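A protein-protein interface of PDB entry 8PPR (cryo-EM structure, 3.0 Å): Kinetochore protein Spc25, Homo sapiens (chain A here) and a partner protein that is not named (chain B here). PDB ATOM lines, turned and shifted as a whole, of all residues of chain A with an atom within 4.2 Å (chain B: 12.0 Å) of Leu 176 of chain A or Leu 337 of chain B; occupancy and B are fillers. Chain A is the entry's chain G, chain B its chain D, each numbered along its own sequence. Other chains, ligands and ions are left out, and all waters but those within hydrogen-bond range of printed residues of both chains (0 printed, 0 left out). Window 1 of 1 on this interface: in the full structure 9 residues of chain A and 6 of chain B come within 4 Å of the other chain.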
ATOM      1  N   LYS A 148      -0.775  14.527 -28.078  1.00  0.00           N
ATOM      2  CA  LYS A 148      -0.567  14.567 -26.638  1.00  0.00           C
ATOM      3  C   LYS A 148       0.715  13.824 -26.299  1.00  0.00           C
ATOM      4  O   LYS A 148       0.957  12.727 -26.813  1.00  0.00           O
ATOM      5  CB  LYS A 148      -1.748  13.947 -25.888  1.00  0.00           C
ATOM      6  CG  LYS A 148      -1.649  14.092 -24.379  1.00  0.00           C
ATOM      7  CD  LYS A 148      -2.980  13.833 -23.700  1.00  0.00           C
ATOM      8  CE  LYS A 148      -2.904  14.161 -22.219  1.00  0.00           C
ATOM      9  NZ  LYS A 148      -4.242  14.467 -21.648  1.00  0.00           N
ATOM     10  N   GLU A 152       1.630  15.801 -19.389  1.00  0.00           N
ATOM     11  CA  GLU A 152       0.368  16.506 -19.604  1.00  0.00           C
ATOM     12  C   GLU A 152       0.600  17.748 -20.468  1.00  0.00           C
ATOM     13  O   GLU A 152       0.263  18.879 -20.113  1.00  0.00           O
ATOM     14  CB  GLU A 152      -0.302  16.848 -18.266  1.00  0.00           C
ATOM     15  CG  GLU A 152      -1.673  17.509 -18.382  1.00  0.00           C
ATOM     16  CD  GLU A 152      -2.309  17.779 -17.034  1.00  0.00           C
ATOM     17  OE1 GLU A 152      -1.674  17.472 -16.004  1.00  0.00           O
ATOM     18  OE2 GLU A 152      -3.445  18.298 -17.006  1.00  0.00           O
ATOM     19  N   LYS A 153       1.224  17.511 -21.616  1.00  0.00           N
ATOM     20  CA  LYS A 153       1.486  18.552 -22.595  1.00  0.00           C
ATOM     21  C   LYS A 153       0.729  18.246 -23.877  1.00  0.00           C
ATOM     22  O   LYS A 153       0.636  17.090 -24.303  1.00  0.00           O
ATOM     23  CB  LYS A 153       2.983  18.677 -22.898  1.00  0.00           C
ATOM     24  CG  LYS A 153       3.782  19.422 -21.845  1.00  0.00           C
ATOM     25  CD  LYS A 153       5.218  19.620 -22.300  1.00  0.00           C
ATOM     26  CE  LYS A 153       6.072  20.237 -21.204  1.00  0.00           C
ATOM     27  NZ  LYS A 153       5.696  21.647 -20.925  1.00  0.00           N
ATOM     28  N   LEU A 154       0.190  19.293 -24.490  1.00  0.00           N
ATOM     29  CA  LEU A 154      -0.512  19.179 -25.763  1.00  0.00           C
ATOM     30  C   LEU A 154       0.363  19.828 -26.825  1.00  0.00           C
ATOM     31  O   LEU A 154       0.605  21.039 -26.788  1.00  0.00           O
ATOM     32  CB  LEU A 154      -1.891  19.829 -25.693  1.00  0.00           C
ATOM     33  CG  LEU A 154      -2.822  19.503 -26.859  1.00  0.00           C
ATOM     34  CD1 LEU A 154      -3.023  18.002 -26.955  1.00  0.00           C
ATOM     35  CD2 LEU A 154      -4.155  20.202 -26.673  1.00  0.00           C
ATOM     36  N   LEU A 174       1.689  23.475 -25.537  1.00  0.00           N
ATOM     37  CA  LEU A 174       0.844  24.132 -24.554  1.00  0.00           C
ATOM     38  C   LEU A 174       0.397  23.109 -23.524  1.00  0.00           C
ATOM     39  O   LEU A 174       0.019  21.986 -23.872  1.00  0.00           O
ATOM     40  CB  LEU A 174      -0.373  24.788 -25.212  1.00  0.00           C
ATOM     41  CG  LEU A 174      -1.309  25.601 -24.310  1.00  0.00           C
ATOM     42  CD1 LEU A 174      -1.879  26.779 -25.077  1.00  0.00           C
ATOM     43  CD2 LEU A 174      -2.440  24.743 -23.757  1.00  0.00           C
ATOM     44  N   HIS A 175       0.448  23.497 -22.254  1.00  0.00           N
ATOM     45  CA  HIS A 175       0.034  22.620 -21.175  1.00  0.00           C
ATOM     46  C   HIS A 175      -0.683  23.431 -20.108  1.00  0.00           C
ATOM     47  O   HIS A 175      -0.394  24.612 -19.898  1.00  0.00           O
ATOM     48  CB  HIS A 175       1.232  21.877 -20.576  1.00  0.00           C
ATOM     49  CG  HIS A 175       2.157  22.750 -19.790  1.00  0.00           C
ATOM     50  ND1 HIS A 175       3.325  23.255 -20.318  1.00  0.00           N
ATOM     51  CD2 HIS A 175       2.096  23.198 -18.515  1.00  0.00           C
ATOM     52  CE1 HIS A 175       3.942  23.980 -19.404  1.00  0.00           C
ATOM     53  NE2 HIS A 175       3.217  23.963 -18.299  1.00  0.00           N
ATOM     54  N   LEU A 176      -1.625  22.779 -19.438  1.00  0.00           N
ATOM     55  CA  LEU A 176      -2.382  23.392 -18.357  1.00  0.00           C
ATOM     56  C   LEU A 176      -1.565  23.290 -17.075  1.00  0.00           C
ATOM     57  O   LEU A 176      -1.176  22.191 -16.666  1.00  0.00           O
ATOM     58  CB  LEU A 176      -3.740  22.708 -18.209  1.00  0.00           C
ATOM     59  CG  LEU A 176      -4.787  23.355 -17.306  1.00  0.00           C
ATOM     60  CD1 LEU A 176      -6.162  23.229 -17.932  1.00  0.00           C
ATOM     61  CD2 LEU A 176      -4.768  22.683 -15.951  1.00  0.00           C
ATOM     62  N   ASN A 177      -1.305  24.432 -16.448  1.00  0.00           N
ATOM     63  CA  ASN A 177      -0.416  24.484 -15.296  1.00  0.00           C
ATOM     64  C   ASN A 177      -1.152  24.005 -14.045  1.00  0.00           C
ATOM     65  O   ASN A 177      -2.289  23.527 -14.101  1.00  0.00           O
ATOM     66  CB  ASN A 177       0.149  25.893 -15.132  1.00  0.00           C
ATOM     67  CG  ASN A 177      -0.886  26.893 -14.644  1.00  0.00           C
ATOM     68  OD1 ASN A 177      -2.086  26.617 -14.638  1.00  0.00           O
ATOM     69  ND2 ASN A 177      -0.422  28.065 -14.230  1.00  0.00           N
ATOM     70  N   ARG A 180      -4.554  25.799 -13.129  1.00  0.00           N
ATOM     71  CA  ARG A 180      -5.624  25.644 -14.114  1.00  0.00           C
ATOM     72  C   ARG A 180      -5.543  26.729 -15.186  1.00  0.00           C
ATOM     73  O   ARG A 180      -6.549  27.308 -15.599  1.00  0.00           O
ATOM     74  CB  ARG A 180      -6.999  25.642 -13.438  1.00  0.00           C
ATOM     75  CG  ARG A 180      -7.151  24.618 -12.321  1.00  0.00           C
ATOM     76  CD  ARG A 180      -6.989  23.194 -12.828  1.00  0.00           C
ATOM     77  NE  ARG A 180      -5.608  22.735 -12.730  1.00  0.00           N
ATOM     78  CZ  ARG A 180      -5.237  21.463 -12.753  1.00  0.00           C
ATOM     79  NH1 ARG A 180      -6.121  20.486 -12.872  1.00  0.00           N
ATOM     80  NH2 ARG A 180      -3.945  21.163 -12.658  1.00  0.00           N
ATOM     81  N   ASP A 181      -4.324  27.000 -15.643  1.00  0.00           N
ATOM     82  CA  ASP A 181      -4.077  28.022 -16.648  1.00  0.00           C
ATOM     83  C   ASP A 181      -3.245  27.437 -17.777  1.00  0.00           C
ATOM     84  O   ASP A 181      -2.303  26.675 -17.538  1.00  0.00           O
ATOM     85  CB  ASP A 181      -3.352  29.232 -16.045  1.00  0.00           C
ATOM     86  CG  ASP A 181      -4.242  30.046 -15.131  1.00  0.00           C
ATOM     87  OD1 ASP A 181      -5.480  29.929 -15.244  1.00  0.00           O
ATOM     88  OD2 ASP A 181      -3.704  30.802 -14.296  1.00  0.00           O
ATOM     89  N   ASP B 329     -18.277  21.180 -25.992  1.00  0.00           N
ATOM     90  CA  ASP B 329     -17.947  21.583 -24.639  1.00  0.00           C
ATOM     91  C   ASP B 329     -17.329  22.981 -24.640  1.00  0.00           C
ATOM     92  O   ASP B 329     -16.858  23.460 -25.675  1.00  0.00           O
ATOM     93  CB  ASP B 329     -17.007  20.559 -23.994  1.00  0.00           C
ATOM     94  CG  ASP B 329     -15.673  20.430 -24.719  1.00  0.00           C
ATOM     95  OD1 ASP B 329     -15.441  21.144 -25.714  1.00  0.00           O
ATOM     96  OD2 ASP B 329     -14.846  19.605 -24.280  1.00  0.00           O
ATOM     97  N   PRO B 330     -17.352  23.674 -23.496  1.00  0.00           N
ATOM     98  CA  PRO B 330     -16.767  25.025 -23.461  1.00  0.00           C
ATOM     99  C   PRO B 330     -15.297  25.068 -23.844  1.00  0.00           C
ATOM    100  O   PRO B 330     -14.862  26.026 -24.493  1.00  0.00           O
ATOM    101  CB  PRO B 330     -16.988  25.460 -22.005  1.00  0.00           C
ATOM    102  CG  PRO B 330     -18.164  24.669 -21.557  1.00  0.00           C
ATOM    103  CD  PRO B 330     -18.041  23.339 -22.238  1.00  0.00           C
ATOM    104  N   SER B 331     -14.519  24.058 -23.466  1.00  0.00           N
ATOM    105  CA  SER B 331     -13.083  24.043 -23.745  1.00  0.00           C
ATOM    106  C   SER B 331     -12.633  22.606 -23.950  1.00  0.00           C
ATOM    107  O   SER B 331     -12.443  21.857 -22.979  1.00  0.00           O
ATOM    108  CB  SER B 331     -12.288  24.705 -22.622  1.00  0.00           C
ATOM    109  OG  SER B 331     -10.907  24.750 -22.935  1.00  0.00           O
ATOM    110  N   PRO B 332     -12.456  22.176 -25.202  1.00  0.00           N
ATOM    111  CA  PRO B 332     -11.868  20.849 -25.441  1.00  0.00           C
ATOM    112  C   PRO B 332     -10.449  20.724 -24.923  1.00  0.00           C
ATOM    113  O   PRO B 332      -9.998  19.604 -24.660  1.00  0.00           O
ATOM    114  CB  PRO B 332     -11.915  20.710 -26.970  1.00  0.00           C
ATOM    115  CG  PRO B 332     -12.902  21.736 -27.430  1.00  0.00           C
ATOM    116  CD  PRO B 332     -12.780  22.868 -26.459  1.00  0.00           C
ATOM    117  N   ALA B 333      -9.731  21.841 -24.774  1.00  0.00           N
ATOM    118  CA  ALA B 333      -8.329  21.779 -24.376  1.00  0.00           C
ATOM    119  C   ALA B 333      -8.168  21.229 -22.964  1.00  0.00           C
ATOM    120  O   ALA B 333      -7.312  20.373 -22.721  1.00  0.00           O
ATOM    121  CB  ALA B 333      -7.692  23.163 -24.486  1.00  0.00           C
ATOM    122  N   ARG B 334      -8.976  21.714 -22.018  1.00  0.00           N
ATOM    123  CA  ARG B 334      -8.875  21.234 -20.644  1.00  0.00           C
ATOM    124  C   ARG B 334      -9.209  19.752 -20.561  1.00  0.00           C
ATOM    125  O   ARG B 334      -8.509  18.978 -19.895  1.00  0.00           O
ATOM    126  CB  ARG B 334      -9.806  22.036 -19.738  1.00  0.00           C
ATOM    127  CG  ARG B 334      -9.824  23.518 -20.028  1.00  0.00           C
ATOM    128  CD  ARG B 334     -10.512  24.285 -18.917  1.00  0.00           C
ATOM    129  NE  ARG B 334      -9.593  24.600 -17.832  1.00  0.00           N
ATOM    130  CZ  ARG B 334      -8.784  25.651 -17.816  1.00  0.00           C
ATOM    131  NH1 ARG B 334      -8.756  26.515 -18.817  1.00  0.00           N
ATOM    132  NH2 ARG B 334      -7.985  25.839 -16.772  1.00  0.00           N
ATOM    133  N   LYS B 335     -10.282  19.342 -21.235  1.00  0.00           N
ATOM    134  CA  LYS B 335     -10.694  17.945 -21.206  1.00  0.00           C
ATOM    135  C   LYS B 335      -9.636  17.048 -21.834  1.00  0.00           C
ATOM    136  O   LYS B 335      -9.369  15.948 -21.342  1.00  0.00           O
ATOM    137  CB  LYS B 335     -12.030  17.790 -21.929  1.00  0.00           C
ATOM    138  CG  LYS B 335     -13.158  18.602 -21.323  1.00  0.00           C
ATOM    139  CD  LYS B 335     -13.881  17.830 -20.238  1.00  0.00           C
ATOM    140  CE  LYS B 335     -15.149  18.550 -19.816  1.00  0.00           C
ATOM    141  NZ  LYS B 335     -14.891  19.989 -19.524  1.00  0.00           N
ATOM    142  N   LEU B 336      -9.033  17.500 -22.934  1.00  0.00           N
ATOM    143  CA  LEU B 336      -7.993  16.714 -23.585  1.00  0.00           C
ATOM    144  C   LEU B 336      -6.740  16.628 -22.724  1.00  0.00           C
ATOM    145  O   LEU B 336      -6.111  15.568 -22.637  1.00  0.00           O
ATOM    146  CB  LEU B 336      -7.673  17.317 -24.950  1.00  0.00           C
ATOM    147  CG  LEU B 336      -6.755  16.506 -25.861  1.00  0.00           C
ATOM    148  CD1 LEU B 336      -7.334  15.122 -26.097  1.00  0.00           C
ATOM    149  CD2 LEU B 336      -6.559  17.237 -27.174  1.00  0.00           C
ATOM    150  N   LEU B 337      -6.358  17.735 -22.081  1.00  0.00           N
ATOM    151  CA  LEU B 337      -5.139  17.745 -21.282  1.00  0.00           C
ATOM    152  C   LEU B 337      -5.296  16.917 -20.015  1.00  0.00           C
ATOM    153  O   LEU B 337      -4.357  16.226 -19.600  1.00  0.00           O
ATOM    154  CB  LEU B 337      -4.751  19.183 -20.941  1.00  0.00           C
ATOM    155  CG  LEU B 337      -3.873  19.886 -21.977  1.00  0.00           C
ATOM    156  CD1 LEU B 337      -3.705  21.357 -21.634  1.00  0.00           C
ATOM    157  CD2 LEU B 337      -2.521  19.199 -22.083  1.00  0.00           C
ATOM    158  N   LYS B 338      -6.472  16.965 -19.388  1.00  0.00           N
ATOM    159  CA  LYS B 338      -6.688  16.215 -18.156  1.00  0.00           C
ATOM    160  C   LYS B 338      -6.698  14.708 -18.375  1.00  0.00           C
ATOM    161  O   LYS B 338      -6.660  13.960 -17.392  1.00  0.00           O
ATOM    162  CB  LYS B 338      -7.997  16.653 -17.499  1.00  0.00           C
ATOM    163  CG  LYS B 338      -9.242  16.198 -18.233  1.00  0.00           C
ATOM    164  CD  LYS B 338     -10.492  16.458 -17.413  1.00  0.00           C
ATOM    165  CE  LYS B 338     -10.763  17.947 -17.288  1.00  0.00           C
ATOM    166  NZ  LYS B 338     -12.049  18.218 -16.590  1.00  0.00           N
ATOM    167  N   LEU B 339      -6.753  14.247 -19.624  1.00  0.00           N
ATOM    168  CA  LEU B 339      -6.701  12.818 -19.897  1.00  0.00           C
ATOM    169  C   LEU B 339      -5.362  12.240 -19.457  1.00  0.00           C
ATOM    170  O   LEU B 339      -4.317  12.886 -19.573  1.00  0.00           O
ATOM    171  CB  LEU B 339      -6.924  12.551 -21.386  1.00  0.00           C
ATOM    172  CG  LEU B 339      -8.279  12.961 -21.965  1.00  0.00           C
ATOM    173  CD1 LEU B 339      -8.431  12.448 -23.388  1.00  0.00           C
ATOM    174  CD2 LEU B 339      -9.413  12.461 -21.085  1.00  0.00           C
ATOM    175  N   GLN B 340      -5.399  11.014 -18.947  1.00  0.00           N
ATOM    176  CA  GLN B 340      -4.195  10.352 -18.460  1.00  0.00           C
ATOM    177  C   GLN B 340      -4.059   8.952 -19.050  1.00  0.00           C
ATOM    178  O   GLN B 340      -3.741   7.998 -18.342  1.00  0.00           O
ATOM    179  CB  GLN B 340      -4.208  10.281 -16.933  1.00  0.00           C
ATOM    180  CG  GLN B 340      -4.146  11.638 -16.253  1.00  0.00           C
ATOM    181  CD  GLN B 340      -4.300  11.542 -14.749  1.00  0.00           C
ATOM    182  OE1 GLN B 340      -4.560  10.469 -14.207  1.00  0.00           O
ATOM    183  NE2 GLN B 340      -4.141  12.669 -14.065  1.00  0.00           N
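The side-chain amino group (NZ) of Lys 148 of chain A is in hydrogen-bond range of the backbone carbonyl oxygen (O) of Leu 339 of chain B (2.6 Å). The backbone carbonyl oxygen (O) of Leu 336 of chain B sits close to the side-chain amino group (NZ) of Lys 148 of chain A, 2.4 Å away. The backbone carbonyl oxygen (O) of Leu 337 of chain B sits close to the side-chain carboxylate (OE2) of Glu 152 of chain A (3.4 Å). NZ of Lys 148 of chain A lies within hydrogen-bond range of O of Leu 337 of chain B. The backbone carbonyl oxygen (O) of Arg 180 of chain A sits close to the guanidinium group (NH2) of Arg 334 of chain B.
Printed residues of chain A that touch a printed residue of chain B: Lys 148, Glu 152, Lys 153, Leu 154, His 175, Leu 176 and Arg 180. Along chain A the printed residues that touch a printed residue of chain B span positions 148 to 180. Of the 12 printed residues of chain B, 4 touch a printed residue of chain A. Hydrophobic or aromatic side chains of chain B within 4 Å of the printed part of chain A: Leu 336, Leu 337 and Leu 339. Among the printed residues, 11 pairs touch across the chains. Among the printed residues, no Asp or Glu carboxylate lies within 4 Å of a Lys or Arg side-chain nitrogen of the other chain.
OD1 of Asn 177 of chain A lies within hydrogen-bond range of N of Arg 180 of chain A (3.0 Å). NZ of Lys 153 of chain A lies within hydrogen-bond range of ND1 of His 175 of chain A, at 2.9 Å. N of Leu 154 of chain A sits at hydrogen-bond distance from O of Leu 174 of chain A, at 2.8 Å.
Printed residues of chain B within 4 Å of Lys 148 of chain A: Leu 336, Leu 337 and Leu 339. Printed residues of chain B within 4 Å of Glu 152 of chain A: Leu 337 (3.2 Å). Of the printed residues of chain B, Lys 153 of chain A touches Leu 337. No residue of chain B comes within 4 Å of Leu 174 of chain A. Of chain B, only Arg 334 (3.4 Å) and Leu 337 (3.3 Å) come within 4 Å of Leu 176 of chain A. Arg 180 of chain A touches one residue of chain B. Asp 329 of chain B touches none of the printed residues of chain A. Of the printed residues of chain A, Arg 334 of chain B touches Leu 176 and Arg 180. Of the printed residues of chain A, Leu 336 of chain B touches Lys 148 and Leu 154. Printed residues of chain A within 4 Å of Leu 339 of chain B: Lys 148 (2.6 Å). The nearest residue of chain B that does not touch Leu 176 of chain A is Ala 333 of chain B (5.7 Å). The nearest printed residue of chain A that does not touch Leu 337 of chain B is Leu 174 of chain A (4.2 Å).
Among the printed residues, pairs that only touch across the chains: Leu 176 of chain A with Leu 337 of chain B (3.3 Å), Leu 176 of chain A with Arg 334 of chain B (3.4 Å), Leu 154 of chain A with Leu 336 of chain B (3.6 Å), Leu 154 of chain A with Leu 337 of chain B (3.6 Å), Lys 153 of chain A with Leu 337 of chain B (3.8 Å) and His 175 of chain A with Leu 337 of chain B (3.97 Å).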
